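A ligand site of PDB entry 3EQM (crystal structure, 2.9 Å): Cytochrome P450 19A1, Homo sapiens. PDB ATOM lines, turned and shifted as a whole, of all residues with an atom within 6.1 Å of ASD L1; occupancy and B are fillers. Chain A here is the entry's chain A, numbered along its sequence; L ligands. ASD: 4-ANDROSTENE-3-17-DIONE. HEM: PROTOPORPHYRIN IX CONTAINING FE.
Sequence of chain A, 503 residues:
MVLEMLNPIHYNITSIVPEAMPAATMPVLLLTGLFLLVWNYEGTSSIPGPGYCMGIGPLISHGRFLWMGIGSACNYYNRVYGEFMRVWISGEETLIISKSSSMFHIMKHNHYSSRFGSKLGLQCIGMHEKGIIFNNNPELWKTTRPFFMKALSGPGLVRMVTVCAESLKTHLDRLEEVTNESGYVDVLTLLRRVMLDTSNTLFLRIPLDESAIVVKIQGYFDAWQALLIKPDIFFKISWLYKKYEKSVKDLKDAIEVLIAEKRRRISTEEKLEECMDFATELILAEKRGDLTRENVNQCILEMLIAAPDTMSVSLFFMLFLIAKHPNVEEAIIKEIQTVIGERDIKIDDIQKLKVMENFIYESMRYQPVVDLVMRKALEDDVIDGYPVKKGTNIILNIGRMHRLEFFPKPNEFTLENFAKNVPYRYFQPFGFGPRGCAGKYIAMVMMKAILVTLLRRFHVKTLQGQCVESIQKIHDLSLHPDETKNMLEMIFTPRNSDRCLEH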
ATOM      1  N   ARG A 115      18.651   0.458  31.710  1.00  0.00           N
ATOM      2  CA  ARG A 115      17.370   0.232  31.025  1.00  0.00           C
ATOM      3  C   ARG A 115      16.344  -0.142  32.090  1.00  0.00           C
ATOM      4  O   ARG A 115      16.597   0.019  33.290  1.00  0.00           O
ATOM      5  CB  ARG A 115      17.485  -0.889  29.964  1.00  0.00           C
ATOM      6  CG  ARG A 115      18.661  -0.738  29.025  1.00  0.00           C
ATOM      7  CD  ARG A 115      18.472  -1.477  27.706  1.00  0.00           C
ATOM      8  NE  ARG A 115      19.693  -1.442  26.913  1.00  0.00           N
ATOM      9  CZ  ARG A 115      20.095  -0.409  26.157  1.00  0.00           C
ATOM     10  NH1 ARG A 115      19.352   0.684  26.060  1.00  0.00           N
ATOM     11  NH2 ARG A 115      21.236  -0.475  25.484  1.00  0.00           N
ATOM     12  N   ILE A 133      22.781  -6.352  27.687  1.00  0.00           N
ATOM     13  CA  ILE A 133      21.664  -5.701  27.002  1.00  0.00           C
ATOM     14  C   ILE A 133      20.634  -5.096  27.978  1.00  0.00           C
ATOM     15  O   ILE A 133      20.363  -3.905  27.939  1.00  0.00           O
ATOM     16  CB  ILE A 133      20.984  -6.607  25.964  1.00  0.00           C
ATOM     17  CG1 ILE A 133      22.014  -7.153  24.978  1.00  0.00           C
ATOM     18  CG2 ILE A 133      19.930  -5.847  25.185  1.00  0.00           C
ATOM     19  CD1 ILE A 133      21.548  -8.394  24.232  1.00  0.00           C
ATOM     20  N   PHE A 134      20.078  -5.933  28.852  1.00  0.00           N
ATOM     21  CA  PHE A 134      19.124  -5.468  29.863  1.00  0.00           C
ATOM     22  C   PHE A 134      19.647  -5.688  31.284  1.00  0.00           C
ATOM     23  O   PHE A 134      18.877  -5.914  32.223  1.00  0.00           O
ATOM     24  CB  PHE A 134      17.733  -6.085  29.652  1.00  0.00           C
ATOM     25  CG  PHE A 134      16.896  -5.346  28.631  1.00  0.00           C
ATOM     26  CD1 PHE A 134      17.024  -5.612  27.277  1.00  0.00           C
ATOM     27  CD2 PHE A 134      15.999  -4.353  29.028  1.00  0.00           C
ATOM     28  CE1 PHE A 134      16.275  -4.912  26.346  1.00  0.00           C
ATOM     29  CE2 PHE A 134      15.253  -3.659  28.104  1.00  0.00           C
ATOM     30  CZ  PHE A 134      15.391  -3.935  26.752  1.00  0.00           C
ATOM     31  N   PHE A 221      14.057 -14.750  21.304  1.00  0.00           N
ATOM     32  CA  PHE A 221      13.665 -13.364  21.093  1.00  0.00           C
ATOM     33  C   PHE A 221      12.194 -13.158  21.411  1.00  0.00           C
ATOM     34  O   PHE A 221      11.812 -12.114  21.931  1.00  0.00           O
ATOM     35  CB  PHE A 221      13.962 -12.867  19.680  1.00  0.00           C
ATOM     36  CG  PHE A 221      13.607 -11.410  19.490  1.00  0.00           C
ATOM     37  CD1 PHE A 221      14.503 -10.409  19.858  1.00  0.00           C
ATOM     38  CD2 PHE A 221      12.354 -11.038  18.991  1.00  0.00           C
ATOM     39  CE1 PHE A 221      14.172  -9.073  19.715  1.00  0.00           C
ATOM     40  CE2 PHE A 221      12.009  -9.705  18.852  1.00  0.00           C
ATOM     41  CZ  PHE A 221      12.918  -8.713  19.207  1.00  0.00           C
ATOM     42  N   TRP A 224      11.669 -13.047  25.244  1.00  0.00           N
ATOM     43  CA  TRP A 224      12.201 -11.757  25.616  1.00  0.00           C
ATOM     44  C   TRP A 224      11.182 -10.667  25.324  1.00  0.00           C
ATOM     45  O   TRP A 224      10.773  -9.925  26.228  1.00  0.00           O
ATOM     46  CB  TRP A 224      13.516 -11.552  24.852  1.00  0.00           C
ATOM     47  CG  TRP A 224      14.212 -10.240  25.010  1.00  0.00           C
ATOM     48  CD1 TRP A 224      13.888  -9.210  25.862  1.00  0.00           C
ATOM     49  CD2 TRP A 224      15.384  -9.817  24.309  1.00  0.00           C
ATOM     50  NE1 TRP A 224      14.781  -8.179  25.715  1.00  0.00           N
ATOM     51  CE2 TRP A 224      15.713  -8.515  24.767  1.00  0.00           C
ATOM     52  CE3 TRP A 224      16.190 -10.405  23.327  1.00  0.00           C
ATOM     53  CZ2 TRP A 224      16.803  -7.799  24.291  1.00  0.00           C
ATOM     54  CZ3 TRP A 224      17.283  -9.688  22.837  1.00  0.00           C
ATOM     55  CH2 TRP A 224      17.573  -8.400  23.328  1.00  0.00           C
ATOM     56  N   GLU A 302      24.192 -13.662  24.642  1.00  0.00           N
ATOM     57  CA  GLU A 302      23.832 -12.352  24.111  1.00  0.00           C
ATOM     58  C   GLU A 302      24.659 -12.003  22.867  1.00  0.00           C
ATOM     59  O   GLU A 302      24.118 -11.463  21.898  1.00  0.00           O
ATOM     60  CB  GLU A 302      23.944 -11.266  25.179  1.00  0.00           C
ATOM     61  CG  GLU A 302      22.887 -11.400  26.299  1.00  0.00           C
ATOM     62  CD  GLU A 302      22.795 -10.195  27.242  1.00  0.00           C
ATOM     63  OE1 GLU A 302      23.561  -9.211  27.091  1.00  0.00           O
ATOM     64  OE2 GLU A 302      21.936 -10.243  28.153  1.00  0.00           O
ATOM     65  N   ILE A 305      23.171 -14.024  19.776  1.00  0.00           N
ATOM     66  CA  ILE A 305      21.848 -13.671  19.281  1.00  0.00           C
ATOM     67  C   ILE A 305      21.810 -12.301  18.611  1.00  0.00           C
ATOM     68  O   ILE A 305      20.988 -12.058  17.735  1.00  0.00           O
ATOM     69  CB  ILE A 305      20.761 -13.735  20.401  1.00  0.00           C
ATOM     70  CG1 ILE A 305      20.990 -12.626  21.446  1.00  0.00           C
ATOM     71  CG2 ILE A 305      20.731 -15.128  21.031  1.00  0.00           C
ATOM     72  CD1 ILE A 305      19.880 -12.478  22.454  1.00  0.00           C
ATOM     73  N   ALA A 306      22.729 -11.421  19.026  1.00  0.00           N
ATOM     74  CA  ALA A 306      22.663 -10.004  18.666  1.00  0.00           C
ATOM     75  C   ALA A 306      22.499  -9.749  17.164  1.00  0.00           C
ATOM     76  O   ALA A 306      21.539  -9.102  16.747  1.00  0.00           O
ATOM     77  CB  ALA A 306      23.872  -9.245  19.218  1.00  0.00           C
ATOM     78  N   ALA A 307      23.425 -10.250  16.362  1.00  0.00           N
ATOM     79  CA  ALA A 307      23.383 -10.016  14.922  1.00  0.00           C
ATOM     80  C   ALA A 307      22.205 -10.734  14.228  1.00  0.00           C
ATOM     81  O   ALA A 307      21.441 -10.087  13.515  1.00  0.00           O
ATOM     82  CB  ALA A 307      24.715 -10.371  14.269  1.00  0.00           C
ATOM     83  N   ASP A 309      19.466 -11.313  15.486  1.00  0.00           N
ATOM     84  CA  ASP A 309      18.259 -10.613  15.861  1.00  0.00           C
ATOM     85  C   ASP A 309      18.055  -9.362  15.034  1.00  0.00           C
ATOM     86  O   ASP A 309      16.989  -9.170  14.439  1.00  0.00           O
ATOM     87  CB  ASP A 309      18.287 -10.252  17.345  1.00  0.00           C
ATOM     88  CG  ASP A 309      17.892 -11.417  18.237  1.00  0.00           C
ATOM     89  OD1 ASP A 309      17.355 -12.422  17.733  1.00  0.00           O
ATOM     90  OD2 ASP A 309      18.128 -11.319  19.464  1.00  0.00           O
ATOM     91  N   THR A 310      19.074  -8.516  14.959  1.00  0.00           N
ATOM     92  CA  THR A 310      18.925  -7.182  14.391  1.00  0.00           C
ATOM     93  C   THR A 310      19.431  -7.022  12.956  1.00  0.00           C
ATOM     94  O   THR A 310      18.780  -6.356  12.154  1.00  0.00           O
ATOM     95  CB  THR A 310      19.601  -6.124  15.266  1.00  0.00           C
ATOM     96  OG1 THR A 310      20.840  -6.658  15.786  1.00  0.00           O
ATOM     97  CG2 THR A 310      18.694  -5.761  16.419  1.00  0.00           C
ATOM     98  N   VAL A 370      15.373  -1.136  15.028  1.00  0.00           N
ATOM     99  CA  VAL A 370      15.507  -0.686  16.399  1.00  0.00           C
ATOM    100  C   VAL A 370      15.093   0.780  16.465  1.00  0.00           C
ATOM    101  O   VAL A 370      15.911   1.691  16.487  1.00  0.00           O
ATOM    102  CB  VAL A 370      16.935  -0.920  16.921  1.00  0.00           C
ATOM    103  CG1 VAL A 370      16.989  -0.724  18.405  1.00  0.00           C
ATOM    104  CG2 VAL A 370      17.420  -2.320  16.555  1.00  0.00           C
ATOM    105  N   LEU A 372      13.274   2.177  18.866  1.00  0.00           N
ATOM    106  CA  LEU A 372      13.145   2.695  20.232  1.00  0.00           C
ATOM    107  C   LEU A 372      14.186   2.160  21.194  1.00  0.00           C
ATOM    108  O   LEU A 372      14.606   1.008  21.103  1.00  0.00           O
ATOM    109  CB  LEU A 372      11.727   2.485  20.776  1.00  0.00           C
ATOM    110  CG  LEU A 372      11.149   1.077  20.798  1.00  0.00           C
ATOM    111  CD1 LEU A 372      11.295   0.453  22.172  1.00  0.00           C
ATOM    112  CD2 LEU A 372       9.692   1.164  20.432  1.00  0.00           C
ATOM    113  N   VAL A 373      14.601   3.026  22.124  1.00  0.00           N
ATOM    114  CA  VAL A 373      15.634   2.707  23.101  1.00  0.00           C
ATOM    115  C   VAL A 373      15.050   2.875  24.494  1.00  0.00           C
ATOM    116  O   VAL A 373      14.425   3.893  24.788  1.00  0.00           O
ATOM    117  CB  VAL A 373      16.883   3.595  22.915  1.00  0.00           C
ATOM    118  CG1 VAL A 373      17.946   3.274  23.943  1.00  0.00           C
ATOM    119  CG2 VAL A 373      17.457   3.438  21.521  1.00  0.00           C
ATOM    120  N   MET A 374      15.249   1.875  25.347  1.00  0.00           N
ATOM    121  CA  MET A 374      14.720   1.912  26.713  1.00  0.00           C
ATOM    122  C   MET A 374      15.805   2.302  27.708  1.00  0.00           C
ATOM    123  O   MET A 374      16.884   1.704  27.727  1.00  0.00           O
ATOM    124  CB  MET A 374      14.097   0.564  27.101  1.00  0.00           C
ATOM    125  CG  MET A 374      12.750   0.284  26.432  1.00  0.00           C
ATOM    126  SD  MET A 374      12.165  -1.436  26.573  1.00  0.00           S
ATOM    127  CE  MET A 374      11.645  -1.498  28.283  1.00  0.00           C
ATOM    128  N   ARG A 375      15.520   3.324  28.511  1.00  0.00           N
ATOM    129  CA  ARG A 375      16.444   3.781  29.562  1.00  0.00           C
ATOM    130  C   ARG A 375      15.735   4.009  30.909  1.00  0.00           C
ATOM    131  O   ARG A 375      14.512   3.899  31.018  1.00  0.00           O
ATOM    132  CB  ARG A 375      17.172   5.056  29.127  1.00  0.00           C
ATOM    133  CG  ARG A 375      17.965   4.978  27.812  1.00  0.00           C
ATOM    134  CD  ARG A 375      19.091   3.971  27.866  1.00  0.00           C
ATOM    135  NE  ARG A 375      20.093   4.192  26.820  1.00  0.00           N
ATOM    136  CZ  ARG A 375      21.178   4.948  26.978  1.00  0.00           C
ATOM    137  NH1 ARG A 375      21.400   5.564  28.128  1.00  0.00           N
ATOM    138  NH2 ARG A 375      22.047   5.083  25.982  1.00  0.00           N
ATOM    139  N   LEU A 477       8.852  -4.865  20.552  1.00  0.00           N
ATOM    140  CA  LEU A 477      10.197  -4.597  21.081  1.00  0.00           C
ATOM    141  C   LEU A 477      11.108  -4.062  19.988  1.00  0.00           C
ATOM    142  O   LEU A 477      11.918  -3.184  20.238  1.00  0.00           O
ATOM    143  CB  LEU A 477      10.815  -5.861  21.675  1.00  0.00           C
ATOM    144  CG  LEU A 477      11.784  -5.789  22.872  1.00  0.00           C
ATOM    145  CD1 LEU A 477      13.048  -6.588  22.597  1.00  0.00           C
ATOM    146  CD2 LEU A 477      12.117  -4.374  23.318  1.00  0.00           C
ATOM    147  N   SER A 478      10.976  -4.606  18.785  1.00  0.00           N
ATOM    148  CA  SER A 478      11.612  -4.055  17.615  1.00  0.00           C
ATOM    149  C   SER A 478      10.562  -3.993  16.511  1.00  0.00           C
ATOM    150  O   SER A 478       9.434  -4.458  16.701  1.00  0.00           O
ATOM    151  CB  SER A 478      12.823  -4.899  17.186  1.00  0.00           C
ATOM    152  OG  SER A 478      12.465  -6.196  16.758  1.00  0.00           O
HETATM  153  C1  ASD L   1      20.141  -5.938  21.295  1.00  0.00           C
HETATM  154  C10 ASD L   1      18.968  -5.187  20.641  1.00  0.00           C
HETATM  155  C11 ASD L   1      19.062  -3.385  22.446  1.00  0.00           C
HETATM  156  C12 ASD L   1      18.325  -2.557  23.493  1.00  0.00           C
HETATM  157  C13 ASD L   1      17.081  -1.962  22.876  1.00  0.00           C
HETATM  158  C14 ASD L   1      16.199  -3.090  22.370  1.00  0.00           C
HETATM  159  C15 ASD L   1      14.809  -2.475  22.200  1.00  0.00           C
HETATM  160  C16 ASD L   1      14.668  -1.559  23.414  1.00  0.00           C
HETATM  161  C17 ASD L   1      16.105  -1.299  23.818  1.00  0.00           C
HETATM  162  C18 ASD L   1      17.423  -0.917  21.801  1.00  0.00           C
HETATM  163  C19 ASD L   1      19.513  -4.193  19.610  1.00  0.00           C
HETATM  164  C2  ASD L   1      20.691  -7.072  20.450  1.00  0.00           C
HETATM  165  C3  ASD L   1      19.536  -7.981  20.081  1.00  0.00           C
HETATM  166  C4  ASD L   1      18.361  -7.438  19.657  1.00  0.00           C
HETATM  167  C5  ASD L   1      18.012  -6.157  19.942  1.00  0.00           C
HETATM  168  C6  ASD L   1      16.627  -5.702  19.535  1.00  0.00           C
HETATM  169  C7  ASD L   1      15.960  -4.995  20.712  1.00  0.00           C
HETATM  170  C8  ASD L   1      16.843  -3.874  21.239  1.00  0.00           C
HETATM  171  C9  ASD L   1      18.191  -4.433  21.731  1.00  0.00           C
HETATM  172  O1  ASD L   1      19.671  -9.199  20.173  1.00  0.00           O
HETATM  173  O2  ASD L   1      16.442  -0.637  24.779  1.00  0.00           O
HETATM  174  CHA HEM L   2      22.361  -1.908  21.973  1.00  0.00           C
HETATM  175  CHB HEM L   2      21.064  -0.742  17.473  1.00  0.00           C
HETATM  176  CHC HEM L   2      23.738  -4.370  15.817  1.00  0.00           C
HETATM  177  CHD HEM L   2      25.232  -5.449  20.253  1.00  0.00           C
HETATM  178  C1A HEM L   2      21.816  -1.247  20.896  1.00  0.00           C
HETATM  179  C2A HEM L   2      21.043  -0.012  20.941  1.00  0.00           C
HETATM  180  C3A HEM L   2      20.694   0.316  19.693  1.00  0.00           C
HETATM  181  C4A HEM L   2      21.238  -0.707  18.826  1.00  0.00           C
HETATM  182  CMA HEM L   2      19.864   1.530  19.236  1.00  0.00           C
HETATM  183  CAA HEM L   2      20.695   0.804  22.201  1.00  0.00           C
HETATM  184  CBA HEM L   2      21.820   1.805  22.454  1.00  0.00           C
HETATM  185  CGA HEM L   2      21.438   2.756  23.564  1.00  0.00           C
HETATM  186  O1A HEM L   2      20.840   2.300  24.576  1.00  0.00           O
HETATM  187  O2A HEM L   2      21.753   3.977  23.444  1.00  0.00           O
HETATM  188  C1B HEM L   2      21.590  -1.688  16.645  1.00  0.00           C
HETATM  189  C2B HEM L   2      21.274  -1.860  15.255  1.00  0.00           C
HETATM  190  C3B HEM L   2      22.024  -2.878  14.800  1.00  0.00           C
HETATM  191  C4B HEM L   2      22.831  -3.344  15.902  1.00  0.00           C
HETATM  192  CMB HEM L   2      20.251  -1.011  14.461  1.00  0.00           C
HETATM  193  CAB HEM L   2      22.075  -3.491  13.386  1.00  0.00           C
HETATM  194  CBB HEM L   2      21.864  -2.738  12.306  1.00  0.00           C
HETATM  195  C1C HEM L   2      24.427  -4.932  16.863  1.00  0.00           C
HETATM  196  C2C HEM L   2      25.434  -5.973  16.749  1.00  0.00           C
HETATM  197  C3C HEM L   2      25.844  -6.272  17.991  1.00  0.00           C
HETATM  198  C4C HEM L   2      25.102  -5.429  18.907  1.00  0.00           C
HETATM  199  CMC HEM L   2      25.909  -6.593  15.418  1.00  0.00           C
HETATM  200  CAC HEM L   2      26.912  -7.300  18.439  1.00  0.00           C
HETATM  201  CBC HEM L   2      27.078  -8.474  17.815  1.00  0.00           C
HETATM  202  C1D HEM L   2      24.566  -4.637  21.126  1.00  0.00           C
HETATM  203  C2D HEM L   2      24.659  -4.761  22.557  1.00  0.00           C
HETATM  204  C3D HEM L   2      23.769  -3.656  23.125  1.00  0.00           C
HETATM  205  C4D HEM L   2      23.223  -2.980  21.954  1.00  0.00           C
HETATM  206  CMD HEM L   2      25.494  -5.803  23.321  1.00  0.00           C
HETATM  207  CAD HEM L   2      23.526  -3.364  24.614  1.00  0.00           C
HETATM  208  CBD HEM L   2      24.430  -2.192  24.998  1.00  0.00           C
HETATM  209  CGD HEM L   2      24.338  -1.853  26.467  1.00  0.00           C
HETATM  210  O1D HEM L   2      25.411  -1.640  27.103  1.00  0.00           O
HETATM  211  O2D HEM L   2      23.195  -1.769  26.996  1.00  0.00           O
HETATM  212  NA  HEM L   2      21.920  -1.642  19.578  1.00  0.00           N
HETATM  213  NB  HEM L   2      22.537  -2.606  17.015  1.00  0.00           N
HETATM  214  NC  HEM L   2      24.243  -4.617  18.185  1.00  0.00           N
HETATM  215  ND  HEM L   2      23.714  -3.586  20.811  1.00  0.00           N
HETATM  216 FE   HEM L   2      23.264  -2.991  18.855  1.00  0.00          FE
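N of Met 374 sits at hydrogen-bond distance from O2 of ASD L1. An oxygen (O1A) of HEM L2 is in salt-bridge range of the guanidinium group of Arg 115 (2.7 Å). O1 of ASD L1 sits close to OD2 of Asp 309 (2.7 Å). An oxygen (O2) of ASD L1 is in hydrogen-bond range of the guanidinium group (NH1) of Arg 115 (3.4 Å). The guanidinium group (NH2) of Arg 375 lies within salt-bridge range of an oxygen (O2A) of HEM L2.
The backbone carbonyl oxygen (O) of Met 374 is in hydrogen-bond range of the guanidinium group (NH1) of Arg 115 (3.1 Å). The side-chain carboxylate of Glu 302 lies within hydrogen-bond range of the backbone NH of Ile 133 (3.0 Å). The guanidinium group of Arg 115 lies within hydrogen-bond range of the backbone carbonyl oxygen of Ile 133, at 2.8 Å. The backbone carbonyl oxygen (O) of Ala 306 lies within hydrogen-bond range of the side-chain hydroxyl (OG1) of Thr 310 (2.7 Å).
Ile 133 touches ASD L1 (CG2 to C11, 3.8 Å). Phe 134 touches ASD L1. CZ3 of Trp 224 touches O1 of ASD L1, 3.6 Å away. Ile 305 touches ASD L1 (CG1 to O1, 3.9 Å). CA of Ala 306 touches O1 of ASD L1, at 3.4 Å. Thr 310 touches ASD L1. CG1 of Val 370 touches C18 of ASD L1, at 3.4 Å. Leu 372 touches ASD L1. Val 373 touches ASD L1. Leu 477 touches ASD L1. Hydrophobic or aromatic side chains within 4 Å of ASD L1: Ile 133, Phe 134, Trp 224, Ile 305, Val 370, Met 374 and Leu 477. 13 residues have an atom within 4 Å of ASD L1: Arg 115, Ile 133, Phe 134, Trp 224, Ile 305, Ala 306, Asp 309, Thr 310, Val 370, Leu 372, Val 373, Met 374 and Leu 477. Along chain A the residues within 4 Å of ASD L1 span positions 115 to 477.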
